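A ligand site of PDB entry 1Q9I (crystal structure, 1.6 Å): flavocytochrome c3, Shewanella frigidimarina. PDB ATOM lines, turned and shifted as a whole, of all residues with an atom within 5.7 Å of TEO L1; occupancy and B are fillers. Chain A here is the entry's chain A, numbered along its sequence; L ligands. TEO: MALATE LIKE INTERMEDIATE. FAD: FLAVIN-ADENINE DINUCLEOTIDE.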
ATOM      1  N   ALA A 168     -29.711  26.438  -2.706  1.00  0.00           N
ATOM      2  CA  ALA A 168     -28.584  27.002  -3.432  1.00  0.00           C
ATOM      3  C   ALA A 168     -27.932  28.130  -2.673  1.00  0.00           C
ATOM      4  O   ALA A 168     -28.617  28.936  -1.998  1.00  0.00           O
ATOM      5  CB  ALA A 168     -28.998  27.437  -4.865  1.00  0.00           C
ATOM      6  N   ALA A 169     -26.599  28.171  -2.704  1.00  0.00           N
ATOM      7  CA  ALA A 169     -25.893  29.202  -1.963  1.00  0.00           C
ATOM      8  C   ALA A 169     -25.150  30.255  -2.824  1.00  0.00           C
ATOM      9  O   ALA A 169     -25.563  31.468  -2.887  1.00  0.00           O
ATOM     10  CB  ALA A 169     -24.958  28.539  -0.946  1.00  0.00           C
ATOM     11  N   GLY A 170     -24.091  29.781  -3.497  1.00  0.00           N
ATOM     12  CA  GLY A 170     -23.060  30.611  -4.082  1.00  0.00           C
ATOM     13  C   GLY A 170     -23.503  31.513  -5.215  1.00  0.00           C
ATOM     14  O   GLY A 170     -22.932  32.579  -5.378  1.00  0.00           O
ATOM     15  N   GLY A 171     -24.503  31.137  -6.010  1.00  0.00           N
ATOM     16  CA  GLY A 171     -25.026  32.114  -6.956  1.00  0.00           C
ATOM     17  C   GLY A 171     -25.567  31.579  -8.272  1.00  0.00           C
ATOM     18  O   GLY A 171     -25.589  30.367  -8.521  1.00  0.00           O
ATOM     19  N   MET A 236     -16.842  31.971  -8.594  1.00  0.00           N
ATOM     20  CA  MET A 236     -16.894  30.535  -8.309  1.00  0.00           C
ATOM     21  C   MET A 236     -15.792  29.818  -9.111  1.00  0.00           C
ATOM     22  O   MET A 236     -15.087  30.457  -9.906  1.00  0.00           O
ATOM     23  CB  MET A 236     -18.272  29.988  -8.689  1.00  0.00           C
ATOM     24  CG  MET A 236     -19.410  30.610  -7.897  1.00  0.00           C
ATOM     25  SD  MET A 236     -19.463  29.949  -6.233  1.00  0.00           S
ATOM     26  CE  MET A 236     -20.507  28.772  -6.501  1.00  0.00           C
ATOM     27  N   GLN A 363     -21.395  14.886 -10.342  1.00  0.00           N
ATOM     28  CA  GLN A 363     -20.505  15.802  -9.633  1.00  0.00           C
ATOM     29  C   GLN A 363     -20.558  15.610  -8.137  1.00  0.00           C
ATOM     30  O   GLN A 363     -21.635  15.570  -7.543  1.00  0.00           O
ATOM     31  CB  GLN A 363     -20.955  17.233  -9.972  1.00  0.00           C
ATOM     32  CG  GLN A 363     -20.268  18.292  -9.092  1.00  0.00           C
ATOM     33  CD  GLN A 363     -20.372  19.663  -9.716  1.00  0.00           C
ATOM     34  OE1 GLN A 363     -21.209  20.478  -9.290  1.00  0.00           O
ATOM     35  NE2 GLN A 363     -19.541  19.909 -10.738  1.00  0.00           N
ATOM     36  N   HIS A 365     -19.606  17.752  -4.926  1.00  0.00           N
ATOM     37  CA  HIS A 365     -19.200  19.063  -4.441  1.00  0.00           C
ATOM     38  C   HIS A 365     -17.969  18.847  -3.585  1.00  0.00           C
ATOM     39  O   HIS A 365     -17.991  17.973  -2.722  1.00  0.00           O
ATOM     40  CB  HIS A 365     -20.300  19.666  -3.580  1.00  0.00           C
ATOM     41  CG  HIS A 365     -20.116  21.122  -3.340  1.00  0.00           C
ATOM     42  ND1 HIS A 365     -19.130  21.638  -2.518  1.00  0.00           N
ATOM     43  CD2 HIS A 365     -20.791  22.194  -3.818  1.00  0.00           C
ATOM     44  CE1 HIS A 365     -19.220  22.951  -2.486  1.00  0.00           C
ATOM     45  NE2 HIS A 365     -20.224  23.314  -3.262  1.00  0.00           N
ATOM     46  N   MET A 375     -23.573  20.924   2.571  1.00  0.00           N
ATOM     47  CA  MET A 375     -22.703  21.674   1.673  1.00  0.00           C
ATOM     48  C   MET A 375     -22.190  22.976   2.310  1.00  0.00           C
ATOM     49  O   MET A 375     -22.954  23.684   2.974  1.00  0.00           O
ATOM     50  CB  MET A 375     -23.466  22.017   0.395  1.00  0.00           C
ATOM     51  CG  MET A 375     -22.582  22.482  -0.712  1.00  0.00           C
ATOM     52  SD  MET A 375     -22.460  24.244  -0.746  1.00  0.00           S
ATOM     53  CE  MET A 375     -24.168  24.779  -0.615  1.00  0.00           C
ATOM     54  N   VAL A 376     -20.895  23.237   2.139  1.00  0.00           N
ATOM     55  CA  VAL A 376     -20.312  24.535   2.455  1.00  0.00           C
ATOM     56  C   VAL A 376     -19.996  25.239   1.153  1.00  0.00           C
ATOM     57  O   VAL A 376     -19.264  24.738   0.306  1.00  0.00           O
ATOM     58  CB  VAL A 376     -19.052  24.413   3.308  1.00  0.00           C
ATOM     59  CG1 VAL A 376     -18.459  25.805   3.510  1.00  0.00           C
ATOM     60  CG2 VAL A 376     -19.371  23.763   4.675  1.00  0.00           C
ATOM     61  N   THR A 377     -20.593  26.405   0.927  1.00  0.00           N
ATOM     62  CA  THR A 377     -20.519  27.004  -0.408  1.00  0.00           C
ATOM     63  C   THR A 377     -19.112  27.261  -0.964  1.00  0.00           C
ATOM     64  O   THR A 377     -18.147  27.647  -0.239  1.00  0.00           O
ATOM     65  CB  THR A 377     -21.413  28.286  -0.482  1.00  0.00           C
ATOM     66  OG1 THR A 377     -21.274  28.849  -1.787  1.00  0.00           O
ATOM     67  CG2 THR A 377     -20.937  29.399   0.505  1.00  0.00           C
ATOM     68  N   GLU A 378     -18.992  27.022  -2.265  1.00  0.00           N
ATOM     69  CA  GLU A 378     -17.800  27.303  -3.018  1.00  0.00           C
ATOM     70  C   GLU A 378     -17.461  28.792  -2.954  1.00  0.00           C
ATOM     71  O   GLU A 378     -16.318  29.191  -3.175  1.00  0.00           O
ATOM     72  CB  GLU A 378     -17.997  26.813  -4.469  1.00  0.00           C
ATOM     73  CG  GLU A 378     -16.817  27.007  -5.382  1.00  0.00           C
ATOM     74  CD  GLU A 378     -16.823  25.954  -6.467  1.00  0.00           C
ATOM     75  OE1 GLU A 378     -16.765  24.756  -6.122  1.00  0.00           O
ATOM     76  OE2 GLU A 378     -16.877  26.331  -7.653  1.00  0.00           O
ATOM     77  N   ALA A 379     -18.491  29.607  -2.672  1.00  0.00           N
ATOM     78  CA  ALA A 379     -18.280  31.038  -2.494  1.00  0.00           C
ATOM     79  C   ALA A 379     -17.345  31.358  -1.307  1.00  0.00           C
ATOM     80  O   ALA A 379     -16.700  32.403  -1.307  1.00  0.00           O
ATOM     81  CB  ALA A 379     -19.618  31.766  -2.363  1.00  0.00           C
ATOM     82  N   ARG A 402     -14.553  21.403 -10.049  1.00  0.00           N
ATOM     83  CA  ARG A 402     -14.941  20.562  -8.912  1.00  0.00           C
ATOM     84  C   ARG A 402     -14.411  19.140  -8.973  1.00  0.00           C
ATOM     85  O   ARG A 402     -14.149  18.533  -7.935  1.00  0.00           O
ATOM     86  CB  ARG A 402     -16.445  20.564  -8.756  1.00  0.00           C
ATOM     87  CG  ARG A 402     -16.897  21.846  -8.136  1.00  0.00           C
ATOM     88  CD  ARG A 402     -18.382  22.005  -8.140  1.00  0.00           C
ATOM     89  NE  ARG A 402     -18.759  23.186  -7.397  1.00  0.00           N
ATOM     90  CZ  ARG A 402     -20.007  23.588  -7.233  1.00  0.00           C
ATOM     91  NH1 ARG A 402     -21.034  22.896  -7.736  1.00  0.00           N
ATOM     92  NH2 ARG A 402     -20.254  24.688  -6.518  1.00  0.00           N
ATOM     93  N   HIS A 504     -23.503  15.563  -5.273  1.00  0.00           N
ATOM     94  CA  HIS A 504     -24.144  16.879  -5.317  1.00  0.00           C
ATOM     95  C   HIS A 504     -25.077  17.094  -6.531  1.00  0.00           C
ATOM     96  O   HIS A 504     -26.182  17.649  -6.369  1.00  0.00           O
ATOM     97  CB  HIS A 504     -23.040  17.931  -5.368  1.00  0.00           C
ATOM     98  CG  HIS A 504     -23.544  19.347  -5.355  1.00  0.00           C
ATOM     99  ND1 HIS A 504     -24.335  19.837  -4.346  1.00  0.00           N
ATOM    100  CD2 HIS A 504     -23.336  20.365  -6.212  1.00  0.00           C
ATOM    101  CE1 HIS A 504     -24.601  21.111  -4.579  1.00  0.00           C
ATOM    102  NE2 HIS A 504     -24.001  21.457  -5.711  1.00  0.00           N
ATOM    103  N   ARG A 544     -19.989  20.260 -14.079  1.00  0.00           N
ATOM    104  CA  ARG A 544     -20.734  21.511 -14.048  1.00  0.00           C
ATOM    105  C   ARG A 544     -19.954  22.612 -13.326  1.00  0.00           C
ATOM    106  O   ARG A 544     -19.355  22.357 -12.291  1.00  0.00           O
ATOM    107  CB  ARG A 544     -22.074  21.306 -13.337  1.00  0.00           C
ATOM    108  CG  ARG A 544     -22.920  22.597 -13.365  1.00  0.00           C
ATOM    109  CD  ARG A 544     -24.320  22.431 -12.840  1.00  0.00           C
ATOM    110  NE  ARG A 544     -24.401  21.979 -11.441  1.00  0.00           N
ATOM    111  CZ  ARG A 544     -24.203  22.758 -10.380  1.00  0.00           C
ATOM    112  NH1 ARG A 544     -23.782  24.009 -10.538  1.00  0.00           N
ATOM    113  NH2 ARG A 544     -24.412  22.259  -9.152  1.00  0.00           N
ATOM    114  N   LEU A 545     -19.999  23.838 -13.840  1.00  0.00           N
ATOM    115  CA  LEU A 545     -19.419  24.965 -13.089  1.00  0.00           C
ATOM    116  C   LEU A 545     -20.333  25.379 -11.970  1.00  0.00           C
ATOM    117  O   LEU A 545     -21.554  25.459 -12.157  1.00  0.00           O
ATOM    118  CB  LEU A 545     -19.205  26.154 -14.011  1.00  0.00           C
ATOM    119  CG  LEU A 545     -18.159  25.939 -15.104  1.00  0.00           C
ATOM    120  CD1 LEU A 545     -17.969  27.254 -15.856  1.00  0.00           C
ATOM    121  CD2 LEU A 545     -16.837  25.418 -14.580  1.00  0.00           C
ATOM    122  N   GLY A 546     -19.759  25.691 -10.802  1.00  0.00           N
ATOM    123  CA  GLY A 546     -20.550  26.310  -9.733  1.00  0.00           C
ATOM    124  C   GLY A 546     -21.259  27.576 -10.239  1.00  0.00           C
ATOM    125  O   GLY A 546     -20.636  28.360 -10.970  1.00  0.00           O
ATOM    126  N   GLY A 547     -22.555  27.727  -9.911  1.00  0.00           N
ATOM    127  CA  GLY A 547     -23.333  28.861 -10.391  1.00  0.00           C
ATOM    128  C   GLY A 547     -24.117  28.561 -11.662  1.00  0.00           C
ATOM    129  O   GLY A 547     -25.075  29.282 -12.038  1.00  0.00           O
ATOM    130  N   ASN A 548     -23.783  27.474 -12.352  1.00  0.00           N
ATOM    131  CA  ASN A 548     -24.429  27.252 -13.644  1.00  0.00           C
ATOM    132  C   ASN A 548     -25.759  26.492 -13.542  1.00  0.00           C
ATOM    133  O   ASN A 548     -26.520  26.461 -14.504  1.00  0.00           O
ATOM    134  CB  ASN A 548     -23.473  26.513 -14.614  1.00  0.00           C
ATOM    135  CG  ASN A 548     -22.755  27.456 -15.580  1.00  0.00           C
ATOM    136  OD1 ASN A 548     -22.924  28.677 -15.526  1.00  0.00           O
ATOM    137  ND2 ASN A 548     -21.955  26.878 -16.470  1.00  0.00           N
ATOM    138  N   ALA A 549     -26.035  25.855 -12.394  1.00  0.00           N
ATOM    139  CA  ALA A 549     -27.296  25.116 -12.291  1.00  0.00           C
ATOM    140  C   ALA A 549     -28.473  26.063 -12.069  1.00  0.00           C
ATOM    141  O   ALA A 549     -29.524  25.867 -12.687  1.00  0.00           O
ATOM    142  CB  ALA A 549     -27.253  24.060 -11.199  1.00  0.00           C
HETATM  143  C1  TEO L   1     -22.194  26.498  -3.854  1.00  0.00           C
HETATM  144  O1A TEO L   1     -22.741  27.456  -3.406  1.00  0.00           O
HETATM  145  O1B TEO L   1     -21.140  25.999  -3.699  1.00  0.00           O
HETATM  146  C2  TEO L   1     -22.938  25.551  -4.892  1.00  0.00           C
HETATM  147  O2  TEO L   1     -23.233  24.342  -4.449  1.00  0.00           O
HETATM  148  C3  TEO L   1     -22.723  25.995  -6.163  1.00  0.00           C
HETATM  149  C4  TEO L   1     -23.245  25.267  -7.201  1.00  0.00           C
HETATM  150  O4A TEO L   1     -23.479  25.623  -8.415  1.00  0.00           O
HETATM  151  O4B TEO L   1     -23.635  23.843  -7.094  1.00  0.00           O
HETATM  152  PA  FAD L   2     -35.067  20.842  -7.874  1.00  0.00           P
HETATM  153  O1A FAD L   2     -34.336  19.713  -7.246  1.00  0.00           O
HETATM  154  O2A FAD L   2     -34.819  22.152  -7.365  1.00  0.00           O
HETATM  155  O5B FAD L   2     -36.593  20.589  -7.833  1.00  0.00           O
HETATM  156  C5B FAD L   2     -37.182  19.395  -8.360  1.00  0.00           C
HETATM  157  C4B FAD L   2     -38.432  19.108  -7.623  1.00  0.00           C
HETATM  158  O4B FAD L   2     -39.262  18.066  -8.271  1.00  0.00           O
HETATM  159  C3B FAD L   2     -38.102  18.600  -6.238  1.00  0.00           C
HETATM  160  O3B FAD L   2     -38.874  19.371  -5.225  1.00  0.00           O
HETATM  161  C2B FAD L   2     -38.716  17.211  -6.139  1.00  0.00           C
HETATM  162  O2B FAD L   2     -39.206  16.606  -4.954  1.00  0.00           O
HETATM  163  C1B FAD L   2     -39.646  17.110  -7.360  1.00  0.00           C
HETATM  164  N9A FAD L   2     -40.093  15.889  -7.899  1.00  0.00           N
HETATM  165  C8A FAD L   2     -39.223  14.903  -8.313  1.00  0.00           C
HETATM  166  N7A FAD L   2     -39.860  13.896  -8.851  1.00  0.00           N
HETATM  167  C5A FAD L   2     -41.202  14.190  -8.809  1.00  0.00           C
HETATM  168  C6A FAD L   2     -42.370  13.575  -9.278  1.00  0.00           C
HETATM  169  N6A FAD L   2     -42.343  12.325  -9.882  1.00  0.00           N
HETATM  170  N1A FAD L   2     -43.505  14.260  -9.062  1.00  0.00           N
HETATM  171  C2A FAD L   2     -43.565  15.418  -8.477  1.00  0.00           C
HETATM  172  N3A FAD L   2     -42.451  16.130  -7.990  1.00  0.00           N
HETATM  173  C4A FAD L   2     -41.318  15.449  -8.236  1.00  0.00           C
HETATM  174  N1  FAD L   2     -26.512  25.432  -8.195  1.00  0.00           N
HETATM  175  C2  FAD L   2     -26.036  26.724  -8.594  1.00  0.00           C
HETATM  176  O2  FAD L   2     -25.953  27.028  -9.772  1.00  0.00           O
HETATM  177  N3  FAD L   2     -25.558  27.668  -7.604  1.00  0.00           N
HETATM  178  C4  FAD L   2     -25.541  27.362  -6.263  1.00  0.00           C
HETATM  179  O4  FAD L   2     -25.506  28.230  -5.519  1.00  0.00           O
HETATM  180  C4X FAD L   2     -26.067  25.966  -5.922  1.00  0.00           C
HETATM  181  N5  FAD L   2     -26.063  25.593  -4.653  1.00  0.00           N
HETATM  182  C5X FAD L   2     -26.552  24.325  -4.230  1.00  0.00           C
HETATM  183  C6  FAD L   2     -26.576  23.969  -2.785  1.00  0.00           C
HETATM  184  C7  FAD L   2     -27.018  22.787  -2.416  1.00  0.00           C
HETATM  185  C7M FAD L   2     -27.087  22.458  -0.955  1.00  0.00           C
HETATM  186  C8  FAD L   2     -27.569  21.928  -3.490  1.00  0.00           C
HETATM  187  C8M FAD L   2     -28.115  20.549  -3.234  1.00  0.00           C
HETATM  188  C9  FAD L   2     -27.540  22.222  -4.864  1.00  0.00           C
HETATM  189  C9A FAD L   2     -27.061  23.462  -5.263  1.00  0.00           C
HETATM  190  N10 FAD L   2     -27.000  23.883  -6.642  1.00  0.00           N
HETATM  191  C10 FAD L   2     -26.508  25.119  -6.976  1.00  0.00           C
HETATM  192  C1' FAD L   2     -27.508  23.010  -7.667  1.00  0.00           C
HETATM  193  C2' FAD L   2     -28.939  23.444  -7.911  1.00  0.00           C
HETATM  194  O2' FAD L   2     -29.630  24.048  -6.735  1.00  0.00           O
HETATM  195  C3' FAD L   2     -29.834  22.226  -8.373  1.00  0.00           C
HETATM  196  O3' FAD L   2     -29.181  21.867  -9.641  1.00  0.00           O
HETATM  197  C4' FAD L   2     -31.285  22.700  -8.793  1.00  0.00           C
HETATM  198  O4' FAD L   2     -31.920  22.648  -7.498  1.00  0.00           O
HETATM  199  C5' FAD L   2     -31.862  22.018  -9.972  1.00  0.00           C
HETATM  200  O5' FAD L   2     -33.156  22.658  -9.870  1.00  0.00           O
HETATM  201  P   FAD L   2     -34.451  21.915 -10.474  1.00  0.00           P
HETATM  202  O1P FAD L   2     -35.528  22.830 -10.541  1.00  0.00           O
HETATM  203  O2P FAD L   2     -34.038  21.247 -11.746  1.00  0.00           O
HETATM  204  O3P FAD L   2     -34.698  20.679  -9.444  1.00  0.00           O
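NH1 of Arg 402 lies within hydrogen-bond range of OE1 of Gln 363 (2.9 Å). The side-chain hydroxyl of Thr 377 sits close to the backbone NH of Gly 170 (3.4 Å). The backbone carbonyl oxygen (O) of Arg 544 is in hydrogen-bond range of the side-chain amide nitrogen (NE2) of Gln 363. N of Ala 379 is in hydrogen-bond range of SD of Met 236. The backbone NH of Ala 379 sits close to the side-chain hydroxyl of Thr 377 (3.0 Å). N of His 504 lies within hydrogen-bond range of O of Gln 363 (2.9 Å). NE2 of His 365 is in hydrogen-bond range of SD of Met 375, at 3.5 Å. The side-chain carboxylate (OE1) of Glu 378 lies within salt-bridge range of the guanidinium group (NE) of Arg 402 (2.8 Å).
N of Asn 548 lies within hydrogen-bond range of O2 of FAD L2 (3.4 Å). The backbone NH of Gly 171 is in hydrogen-bond range of an oxygen (O4) of FAD L2. The backbone carbonyl oxygen of Gly 171 is in hydrogen-bond range of a nitrogen (N3) of FAD L2, at 2.9 Å. The backbone NH (N) of Glu 378 is in hydrogen-bond range of an oxygen (O1B) of TEO L1, 2.8 Å away. NE2 of His 365 is in hydrogen-bond range of O1B of TEO L1. NH2 of Arg 402 lies within salt-bridge range of O1B of TEO L1. N of Gly 547 sits at hydrogen-bond distance from O4A of TEO L1, 2.7 Å away. An oxygen (O1A) of TEO L1 lies within hydrogen-bond range of the side-chain hydroxyl (OG1) of Thr 377 (2.6 Å). An oxygen (O4B) of TEO L1 sits at hydrogen-bond distance from a ring nitrogen (NE2) of His 504 (2.8 Å). An oxygen (O4A) of TEO L1 sits at hydrogen-bond distance from the guanidinium group (NH1) of Arg 544, at 2.7 Å. N of Gly 170 lies within hydrogen-bond range of O4 of FAD L2, at 2.9 Å. An oxygen (O4) of FAD L2 lies within hydrogen-bond range of the backbone NH of Ala 169 (3.0 Å). The backbone NH (N) of Gly 547 sits close to an oxygen (O2) of FAD L2 (3.5 Å). The backbone NH (N) of Gly 170 sits at hydrogen-bond distance from an oxygen (O1A) of TEO L1, at 2.7 Å. N of Ala 549 sits at hydrogen-bond distance from O2 of FAD L2, 2.9 Å away. O2 of TEO L1 is in hydrogen-bond range of SD of Met 375 (3.8 Å).
Residues that only touch TEO L1: Gly 546 (3.3 Å), Ala 169 (3.5 Å) and Met 236 (3.6 Å). Of the 20 residues printed, 12 come within 4 Å of TEO L1.
An oxygen (O4A) of TEO L1 sits close to a nitrogen (N3) of FAD L2 (3.0 Å).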
